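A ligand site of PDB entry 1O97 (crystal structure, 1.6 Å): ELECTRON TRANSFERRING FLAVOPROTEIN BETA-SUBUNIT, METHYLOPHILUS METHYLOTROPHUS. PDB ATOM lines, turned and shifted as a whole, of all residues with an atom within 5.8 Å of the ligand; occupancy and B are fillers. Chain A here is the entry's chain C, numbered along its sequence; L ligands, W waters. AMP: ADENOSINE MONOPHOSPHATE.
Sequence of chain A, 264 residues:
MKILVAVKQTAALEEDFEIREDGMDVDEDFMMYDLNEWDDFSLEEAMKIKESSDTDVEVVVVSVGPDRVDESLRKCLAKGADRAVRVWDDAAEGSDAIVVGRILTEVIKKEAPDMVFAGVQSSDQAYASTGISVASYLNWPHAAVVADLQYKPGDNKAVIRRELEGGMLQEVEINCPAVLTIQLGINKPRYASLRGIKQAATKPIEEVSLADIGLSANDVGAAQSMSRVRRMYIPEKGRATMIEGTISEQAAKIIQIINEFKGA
OD1 of Asp 39 sits at hydrogen-bond distance from O3' of the ligand (2.6 Å). The backbone carbonyl oxygen (O) of Ala 6 sits at hydrogen-bond distance from an oxygen (O2') of the ligand (2.7 Å). The backbone NH (N) of Ser 129 is in hydrogen-bond range of an oxygen (O2P) of the ligand (2.7 Å). The backbone NH of Thr 130 lies within hydrogen-bond range of an oxygen (O2P) of the ligand. OG1 of Thr 130 is in hydrogen-bond range of O1P of the ligand, at 3.0 Å. The backbone NH of Ser 122 sits at hydrogen-bond distance from an oxygen (O3P) of the ligand, at 2.8 Å. An oxygen (O3P) of the ligand is in hydrogen-bond range of the side-chain hydroxyl (OG) of Ser 122, 3.0 Å away. A nitrogen (N1) of the ligand sits at hydrogen-bond distance from the backbone NH of Val 64 (3.0 Å). A nitrogen (N6) of the ligand sits at hydrogen-bond distance from the backbone carbonyl oxygen (O) of Val 64, at 2.9 Å. An oxygen (O3P) of the ligand sits at hydrogen-bond distance from the backbone NH (N) of Ala 128. The backbone NH (N) of Gly 119 is in hydrogen-bond range of an oxygen (O2') of the ligand (2.9 Å). The side-chain amide nitrogen of Asn 36 is in hydrogen-bond range of an oxygen (O3') of the ligand (2.9 Å). O3P of the ligand is in hydrogen-bond range of N of Tyr 127 (3.0 Å).
The side-chain carboxylate (OD2) of Asp 39 lies within hydrogen-bond range of the backbone NH (N) of Lys 8 (2.8 Å). The backbone carbonyl oxygen (O) of Phe 117 sits at hydrogen-bond distance from the backbone NH (N) of Ala 6. OG of Ser 129 lies within hydrogen-bond range of O of Tyr 127, 3.1 Å away. OG of Ser 122 is in hydrogen-bond range of N of Ala 126 (3.1 Å). N of Val 7 sits at hydrogen-bond distance from O of Val 62. The backbone carbonyl oxygen (O) of Val 7 sits at hydrogen-bond distance from the side-chain hydroxyl (OG) of Ser 63 (2.6 Å). The side-chain amide nitrogen of Asn 36 is in hydrogen-bond range of the backbone carbonyl oxygen of Gln 121. The backbone NH (N) of Asn 36 sits at hydrogen-bond distance from the backbone carbonyl oxygen (O) of Lys 8, at 2.9 Å.
The backbone carbonyl oxygen (O) of Val 7 lies close to a nitrogen (N1) of the ligand (3.2 Å). Lys 8 touches the ligand (CD to N7, 3.6 Å). Val 62 touches the ligand (O to C2, 3.5 Å). Ser 63 touches the ligand (OG to N1, 3.6 Å). Val 100 touches the ligand. Leu 104 touches the ligand. CA of Ala 118 touches O2' of the ligand, 3.2 Å away. CA of Gln 121 touches O5' of the ligand, 3.3 Å away. Ala 126 touches the ligand (C to O3P, 3.8 Å). Hydrophobic or aromatic side chains that line the ligand: Ala 6, Val 64, Val 100, Leu 104, Ala 118 and Tyr 127. Of the 26 residues printed, 19 come within 4 Å of the ligand. The nearest printed residue that does not touch the ligand is Val 120 (4.3 Å).
Water W4 lies within hydrogen-bond range of OG1 of Thr 130 (2.8 Å) and N7 of the ligand (3.0 Å). Water W3 lies within hydrogen-bond range of OD1 of Asp 39 (2.6 Å), O of Ala 6 (2.7 Å), N of Gly 119 (3.2 Å) and O2' of the ligand (3.4 Å).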
ATOM      1  N   ALA A   6       1.293 -23.489 -16.159  1.00  0.00           N
ATOM      2  CA  ALA A   6       0.882 -22.834 -17.440  1.00  0.00           C
ATOM      3  C   ALA A   6       1.907 -21.757 -17.766  1.00  0.00           C
ATOM      4  O   ALA A   6       2.215 -20.919 -16.931  1.00  0.00           O
ATOM      5  CB  ALA A   6      -0.452 -22.172 -17.263  1.00  0.00           C
ATOM      6  N   VAL A   7       2.477 -21.842 -18.977  1.00  0.00           N
ATOM      7  CA  VAL A   7       3.472 -20.845 -19.373  1.00  0.00           C
ATOM      8  C   VAL A   7       3.070 -20.174 -20.701  1.00  0.00           C
ATOM      9  O   VAL A   7       2.475 -20.810 -21.589  1.00  0.00           O
ATOM     10  CB  VAL A   7       4.901 -21.476 -19.500  1.00  0.00           C
ATOM     11  CG1 VAL A   7       5.361 -22.044 -18.105  1.00  0.00           C
ATOM     12  CG2 VAL A   7       4.947 -22.563 -20.602  1.00  0.00           C
ATOM     13  N   LYS A   8       3.468 -18.909 -20.780  1.00  0.00           N
ATOM     14  CA  LYS A   8       3.209 -18.085 -21.983  1.00  0.00           C
ATOM     15  C   LYS A   8       4.522 -17.627 -22.598  1.00  0.00           C
ATOM     16  O   LYS A   8       5.405 -17.100 -21.901  1.00  0.00           O
ATOM     17  CB  LYS A   8       2.370 -16.860 -21.647  1.00  0.00           C
ATOM     18  CG  LYS A   8       1.820 -16.129 -22.897  1.00  0.00           C
ATOM     19  CD  LYS A   8       1.204 -14.811 -22.557  1.00  0.00           C
ATOM     20  CE  LYS A   8       0.699 -14.120 -23.849  1.00  0.00           C
ATOM     21  NZ  LYS A   8       0.026 -12.815 -23.555  1.00  0.00           N
ATOM     22  N   ASN A  36       7.628 -15.671 -20.784  1.00  0.00           N
ATOM     23  CA  ASN A  36       7.193 -14.661 -19.852  1.00  0.00           C
ATOM     24  C   ASN A  36       8.046 -14.671 -18.564  1.00  0.00           C
ATOM     25  O   ASN A  36       8.298 -15.736 -18.007  1.00  0.00           O
ATOM     26  CB  ASN A  36       5.721 -14.952 -19.500  1.00  0.00           C
ATOM     27  CG  ASN A  36       5.110 -13.859 -18.658  1.00  0.00           C
ATOM     28  OD1 ASN A  36       5.490 -12.723 -18.757  1.00  0.00           O
ATOM     29  ND2 ASN A  36       4.161 -14.231 -17.759  1.00  0.00           N
ATOM     30  N   TRP A  38       7.425 -13.905 -15.519  1.00  0.00           N
ATOM     31  CA  TRP A  38       6.776 -14.568 -14.351  1.00  0.00           C
ATOM     32  C   TRP A  38       6.906 -16.068 -14.369  1.00  0.00           C
ATOM     33  O   TRP A  38       6.912 -16.714 -13.323  1.00  0.00           O
ATOM     34  CB  TRP A  38       5.297 -14.158 -14.215  1.00  0.00           C
ATOM     35  CG  TRP A  38       5.142 -12.835 -13.558  1.00  0.00           C
ATOM     36  CD1 TRP A  38       4.865 -12.594 -12.196  1.00  0.00           C
ATOM     37  CD2 TRP A  38       5.301 -11.531 -14.151  1.00  0.00           C
ATOM     38  NE1 TRP A  38       4.854 -11.258 -11.957  1.00  0.00           N
ATOM     39  CE2 TRP A  38       5.109 -10.568 -13.135  1.00  0.00           C
ATOM     40  CE3 TRP A  38       5.584 -11.092 -15.452  1.00  0.00           C
ATOM     41  CZ2 TRP A  38       5.181  -9.211 -13.363  1.00  0.00           C
ATOM     42  CZ3 TRP A  38       5.644  -9.715 -15.685  1.00  0.00           C
ATOM     43  CH2 TRP A  38       5.435  -8.799 -14.648  1.00  0.00           C
ATOM     44  N   ASP A  39       6.977 -16.646 -15.544  1.00  0.00           N
ATOM     45  CA  ASP A  39       7.015 -18.088 -15.677  1.00  0.00           C
ATOM     46  C   ASP A  39       8.346 -18.712 -15.247  1.00  0.00           C
ATOM     47  O   ASP A  39       8.370 -19.871 -14.830  1.00  0.00           O
ATOM     48  CB  ASP A  39       6.606 -18.498 -17.084  1.00  0.00           C
ATOM     49  CG  ASP A  39       5.153 -18.115 -17.374  1.00  0.00           C
ATOM     50  OD1 ASP A  39       4.346 -18.088 -16.404  1.00  0.00           O
ATOM     51  OD2 ASP A  39       4.709 -17.809 -18.501  1.00  0.00           O
ATOM     52  N   VAL A  62       2.605 -26.319 -19.700  1.00  0.00           N
ATOM     53  CA  VAL A  62       1.586 -26.351 -20.725  1.00  0.00           C
ATOM     54  C   VAL A  62       1.453 -24.941 -21.299  1.00  0.00           C
ATOM     55  O   VAL A  62       1.347 -23.950 -20.556  1.00  0.00           O
ATOM     56  CB  VAL A  62       0.179 -26.781 -20.114  1.00  0.00           C
ATOM     57  CG1 VAL A  62      -0.888 -26.795 -21.244  1.00  0.00           C
ATOM     58  CG2 VAL A  62       0.320 -28.168 -19.543  1.00  0.00           C
ATOM     59  N   SER A  63       1.414 -24.812 -22.654  1.00  0.00           N
ATOM     60  CA  SER A  63       1.197 -23.481 -23.192  1.00  0.00           C
ATOM     61  C   SER A  63       0.192 -23.621 -24.347  1.00  0.00           C
ATOM     62  O   SER A  63       0.166 -24.613 -25.028  1.00  0.00           O
ATOM     63  CB  SER A  63       2.530 -22.919 -23.769  1.00  0.00           C
ATOM     64  OG  SER A  63       2.363 -21.552 -24.079  1.00  0.00           O
ATOM     65  N   VAL A  64      -0.669 -22.626 -24.504  1.00  0.00           N
ATOM     66  CA  VAL A  64      -1.593 -22.561 -25.627  1.00  0.00           C
ATOM     67  C   VAL A  64      -0.991 -21.562 -26.623  1.00  0.00           C
ATOM     68  O   VAL A  64      -0.871 -20.366 -26.331  1.00  0.00           O
ATOM     69  CB  VAL A  64      -2.924 -22.028 -25.169  1.00  0.00           C
ATOM     70  CG1 VAL A  64      -3.919 -21.950 -26.334  1.00  0.00           C
ATOM     71  CG2 VAL A  64      -3.525 -22.959 -24.098  1.00  0.00           C
ATOM     72  N   GLY A  65      -0.576 -22.058 -27.785  1.00  0.00           N
ATOM     73  CA  GLY A  65       0.032 -21.145 -28.730  1.00  0.00           C
ATOM     74  C   GLY A  65       0.466 -21.911 -29.991  1.00  0.00           C
ATOM     75  O   GLY A  65       0.549 -23.125 -29.988  1.00  0.00           O
ATOM     76  N   ALA A  97      -7.813 -13.825 -22.469  1.00  0.00           N
ATOM     77  CA  ALA A  97      -7.386 -14.523 -21.230  1.00  0.00           C
ATOM     78  C   ALA A  97      -8.437 -15.490 -20.738  1.00  0.00           C
ATOM     79  O   ALA A  97      -8.096 -16.537 -20.198  1.00  0.00           O
ATOM     80  CB  ALA A  97      -7.070 -13.541 -20.152  1.00  0.00           C
ATOM     81  N   VAL A 100      -8.358 -18.539 -23.147  1.00  0.00           N
ATOM     82  CA  VAL A 100      -7.182 -19.308 -22.814  1.00  0.00           C
ATOM     83  C   VAL A 100      -7.412 -20.087 -21.506  1.00  0.00           C
ATOM     84  O   VAL A 100      -7.037 -21.236 -21.410  1.00  0.00           O
ATOM     85  CB  VAL A 100      -5.896 -18.447 -22.781  1.00  0.00           C
ATOM     86  CG1 VAL A 100      -4.708 -19.300 -22.260  1.00  0.00           C
ATOM     87  CG2 VAL A 100      -5.551 -17.974 -24.263  1.00  0.00           C
ATOM     88  N   LEU A 104      -6.956 -24.125 -21.211  1.00  0.00           N
ATOM     89  CA  LEU A 104      -6.008 -24.710 -20.239  1.00  0.00           C
ATOM     90  C   LEU A 104      -6.773 -25.663 -19.318  1.00  0.00           C
ATOM     91  O   LEU A 104      -6.272 -26.732 -19.007  1.00  0.00           O
ATOM     92  CB  LEU A 104      -5.322 -23.638 -19.377  1.00  0.00           C
ATOM     93  CG  LEU A 104      -4.222 -22.801 -20.066  1.00  0.00           C
ATOM     94  CD1 LEU A 104      -3.799 -21.557 -19.319  1.00  0.00           C
ATOM     95  CD2 LEU A 104      -2.975 -23.683 -20.364  1.00  0.00           C
ATOM     96  N   PHE A 117       0.152 -23.857 -11.164  1.00  0.00           N
ATOM     97  CA  PHE A 117       0.773 -22.581 -11.030  1.00  0.00           C
ATOM     98  C   PHE A 117       0.669 -21.778 -12.326  1.00  0.00           C
ATOM     99  O   PHE A 117       0.759 -22.357 -13.435  1.00  0.00           O
ATOM    100  CB  PHE A 117       2.260 -22.687 -10.740  1.00  0.00           C
ATOM    101  CG  PHE A 117       2.633 -23.357  -9.440  1.00  0.00           C
ATOM    102  CD1 PHE A 117       1.679 -23.609  -8.430  1.00  0.00           C
ATOM    103  CD2 PHE A 117       3.964 -23.706  -9.212  1.00  0.00           C
ATOM    104  CE1 PHE A 117       2.072 -24.246  -7.239  1.00  0.00           C
ATOM    105  CE2 PHE A 117       4.376 -24.323  -8.047  1.00  0.00           C
ATOM    106  CZ  PHE A 117       3.412 -24.578  -7.023  1.00  0.00           C
ATOM    107  N   ALA A 118       0.384 -20.492 -12.178  1.00  0.00           N
ATOM    108  CA  ALA A 118       0.394 -19.545 -13.357  1.00  0.00           C
ATOM    109  C   ALA A 118       1.100 -18.301 -12.954  1.00  0.00           C
ATOM    110  O   ALA A 118       1.267 -18.024 -11.771  1.00  0.00           O
ATOM    111  CB  ALA A 118      -1.058 -19.143 -13.722  1.00  0.00           C
ATOM    112  N   GLY A 119       1.618 -17.486 -13.922  1.00  0.00           N
ATOM    113  CA  GLY A 119       2.232 -16.239 -13.507  1.00  0.00           C
ATOM    114  C   GLY A 119       1.195 -15.186 -13.064  1.00  0.00           C
ATOM    115  O   GLY A 119       0.059 -15.246 -13.495  1.00  0.00           O
ATOM    116  N   VAL A 120       1.571 -14.214 -12.259  1.00  0.00           N
ATOM    117  CA  VAL A 120       0.651 -13.085 -11.910  1.00  0.00           C
ATOM    118  C   VAL A 120       0.094 -12.381 -13.179  1.00  0.00           C
ATOM    119  O   VAL A 120      -1.072 -12.140 -13.249  1.00  0.00           O
ATOM    120  CB  VAL A 120       1.351 -12.070 -10.992  1.00  0.00           C
ATOM    121  CG1 VAL A 120       0.630 -10.726 -10.893  1.00  0.00           C
ATOM    122  CG2 VAL A 120       1.523 -12.672  -9.599  1.00  0.00           C
ATOM    123  N   GLN A 121       1.002 -12.091 -14.134  1.00  0.00           N
ATOM    124  CA  GLN A 121       0.541 -11.450 -15.397  1.00  0.00           C
ATOM    125  C   GLN A 121       1.565 -11.716 -16.492  1.00  0.00           C
ATOM    126  O   GLN A 121       2.642 -12.257 -16.212  1.00  0.00           O
ATOM    127  CB  GLN A 121       0.425  -9.953 -15.200  1.00  0.00           C
ATOM    128  CG  GLN A 121       1.745  -9.215 -14.949  1.00  0.00           C
ATOM    129  CD  GLN A 121       1.510  -7.720 -14.776  1.00  0.00           C
ATOM    130  OE1 GLN A 121       2.247  -6.910 -15.333  1.00  0.00           O
ATOM    131  NE2 GLN A 121       0.486  -7.345 -14.022  1.00  0.00           N
ATOM    132  N   SER A 122       1.168 -11.349 -17.710  1.00  0.00           N
ATOM    133  CA  SER A 122       2.100 -11.455 -18.882  1.00  0.00           C
ATOM    134  C   SER A 122       2.775 -10.111 -19.066  1.00  0.00           C
ATOM    135  O   SER A 122       2.198  -9.060 -18.838  1.00  0.00           O
ATOM    136  CB  SER A 122       1.306 -11.886 -20.114  1.00  0.00           C
ATOM    137  OG  SER A 122       0.189 -11.045 -20.321  1.00  0.00           O
ATOM    138  N   GLN A 125       0.804  -8.232 -22.571  1.00  0.00           N
ATOM    139  CA  GLN A 125      -0.541  -7.655 -22.407  1.00  0.00           C
ATOM    140  C   GLN A 125      -0.946  -7.366 -20.968  1.00  0.00           C
ATOM    141  O   GLN A 125      -1.835  -6.522 -20.755  1.00  0.00           O
ATOM    142  CB  GLN A 125      -1.560  -8.583 -23.060  1.00  0.00           C
ATOM    143  CG  GLN A 125      -1.229  -8.922 -24.558  1.00  0.00           C
ATOM    144  CD  GLN A 125      -0.522  -7.797 -25.412  1.00  0.00           C
ATOM    145  OE1 GLN A 125      -0.689  -6.605 -25.233  1.00  0.00           O
ATOM    146  NE2 GLN A 125       0.225  -8.243 -26.403  1.00  0.00           N
ATOM    147  N   ALA A 126      -0.275  -8.007 -19.995  1.00  0.00           N
ATOM    148  CA  ALA A 126      -0.550  -7.705 -18.552  1.00  0.00           C
ATOM    149  C   ALA A 126      -2.036  -7.707 -18.264  1.00  0.00           C
ATOM    150  O   ALA A 126      -2.528  -6.753 -17.620  1.00  0.00           O
ATOM    151  CB  ALA A 126       0.129  -6.409 -18.128  1.00  0.00           C
ATOM    152  N   TYR A 127      -2.708  -8.777 -18.654  1.00  0.00           N
ATOM    153  CA  TYR A 127      -4.139  -8.953 -18.320  1.00  0.00           C
ATOM    154  C   TYR A 127      -4.335  -9.205 -16.824  1.00  0.00           C
ATOM    155  O   TYR A 127      -5.302  -8.725 -16.253  1.00  0.00           O
ATOM    156  CB  TYR A 127      -4.802 -10.105 -19.073  1.00  0.00           C
ATOM    157  CG  TYR A 127      -4.769  -9.930 -20.591  1.00  0.00           C
ATOM    158  CD1 TYR A 127      -4.271 -10.903 -21.395  1.00  0.00           C
ATOM    159  CD2 TYR A 127      -5.278  -8.780 -21.212  1.00  0.00           C
ATOM    160  CE1 TYR A 127      -4.267 -10.794 -22.781  1.00  0.00           C
ATOM    161  CE2 TYR A 127      -5.237  -8.628 -22.625  1.00  0.00           C
ATOM    162  CZ  TYR A 127      -4.735  -9.654 -23.402  1.00  0.00           C
ATOM    163  OH  TYR A 127      -4.682  -9.621 -24.827  1.00  0.00           O
ATOM    164  N   ALA A 128      -3.408  -9.968 -16.258  1.00  0.00           N
ATOM    165  CA  ALA A 128      -3.509 -10.439 -14.865  1.00  0.00           C
ATOM    166  C   ALA A 128      -4.851 -11.096 -14.668  1.00  0.00           C
ATOM    167  O   ALA A 128      -5.541 -10.834 -13.660  1.00  0.00           O
ATOM    168  CB  ALA A 128      -3.288  -9.285 -13.848  1.00  0.00           C
ATOM    169  N   SER A 129      -5.169 -12.009 -15.585  1.00  0.00           N
ATOM    170  CA  SER A 129      -6.485 -12.640 -15.640  1.00  0.00           C
ATOM    171  C   SER A 129      -6.499 -14.126 -15.896  1.00  0.00           C
ATOM    172  O   SER A 129      -7.440 -14.830 -15.548  1.00  0.00           O
ATOM    173  CB  SER A 129      -7.269 -12.018 -16.797  1.00  0.00           C
ATOM    174  OG  SER A 129      -7.635 -10.705 -16.404  1.00  0.00           O
ATOM    175  N   THR A 130      -5.476 -14.634 -16.577  1.00  0.00           N
ATOM    176  CA  THR A 130      -5.565 -15.979 -17.105  1.00  0.00           C
ATOM    177  C   THR A 130      -5.601 -17.052 -16.011  1.00  0.00           C
ATOM    178  O   THR A 130      -6.418 -17.972 -16.065  1.00  0.00           O
ATOM    179  CB  THR A 130      -4.413 -16.238 -18.119  1.00  0.00           C
ATOM    180  OG1 THR A 130      -4.474 -15.220 -19.145  1.00  0.00           O
ATOM    181  CG2 THR A 130      -4.606 -17.587 -18.828  1.00  0.00           C
ATOM    182  N   GLY A 131      -4.699 -16.923 -15.045  1.00  0.00           N
ATOM    183  CA  GLY A 131      -4.601 -17.999 -14.034  1.00  0.00           C
ATOM    184  C   GLY A 131      -5.855 -18.106 -13.185  1.00  0.00           C
ATOM    185  O   GLY A 131      -6.372 -19.223 -12.928  1.00  0.00           O
HETATM  186  P   AMP L   1      -2.055 -12.879 -18.044  1.00  0.00           P
HETATM  187  O1P AMP L   1      -2.062 -13.527 -19.373  1.00  0.00           O
HETATM  188  O2P AMP L   1      -3.361 -12.997 -17.391  1.00  0.00           O
HETATM  189  O3P AMP L   1      -1.634 -11.490 -17.975  1.00  0.00           O
HETATM  190  O5' AMP L   1      -1.005 -13.765 -17.201  1.00  0.00           O
HETATM  191  C5' AMP L   1       0.111 -14.477 -17.662  1.00  0.00           C
HETATM  192  C4' AMP L   1       0.030 -15.875 -17.018  1.00  0.00           C
HETATM  193  O4' AMP L   1      -1.110 -16.658 -17.429  1.00  0.00           O
HETATM  194  C3' AMP L   1       1.221 -16.600 -17.586  1.00  0.00           C
HETATM  195  O3' AMP L   1       2.401 -16.369 -16.828  1.00  0.00           O
HETATM  196  C2' AMP L   1       0.793 -18.011 -17.701  1.00  0.00           C
HETATM  197  O2' AMP L   1       0.817 -18.708 -16.441  1.00  0.00           O
HETATM  198  C1' AMP L   1      -0.728 -17.859 -18.027  1.00  0.00           C
HETATM  199  N9  AMP L   1      -0.943 -17.736 -19.508  1.00  0.00           N
HETATM  200  C8  AMP L   1      -1.346 -16.614 -20.210  1.00  0.00           C
HETATM  201  N7  AMP L   1      -1.449 -17.004 -21.501  1.00  0.00           N
HETATM  202  C5  AMP L   1      -1.123 -18.313 -21.616  1.00  0.00           C
HETATM  203  C6  AMP L   1      -1.026 -19.196 -22.700  1.00  0.00           C
HETATM  204  N6  AMP L   1      -1.305 -18.780 -23.980  1.00  0.00           N
HETATM  205  N1  AMP L   1      -0.631 -20.503 -22.449  1.00  0.00           N
HETATM  206  C2  AMP L   1      -0.392 -20.934 -21.151  1.00  0.00           C
HETATM  207  N3  AMP L   1      -0.438 -20.052 -20.073  1.00  0.00           N
HETATM  208  C4  AMP L   1      -0.799 -18.774 -20.350  1.00  0.00           C
HETATM  209  O   HOH W   1      -2.619 -14.783 -14.688  1.00  0.00           O
HETATM  210  O   HOH W   2      -2.113 -16.222 -25.314  1.00  0.00           O
HETATM  211  O   HOH W   3       3.458 -19.923 -14.725  1.00  0.00           O
HETATM  212  O   HOH W   4      -3.953 -15.433 -21.922  1.00  0.00           O
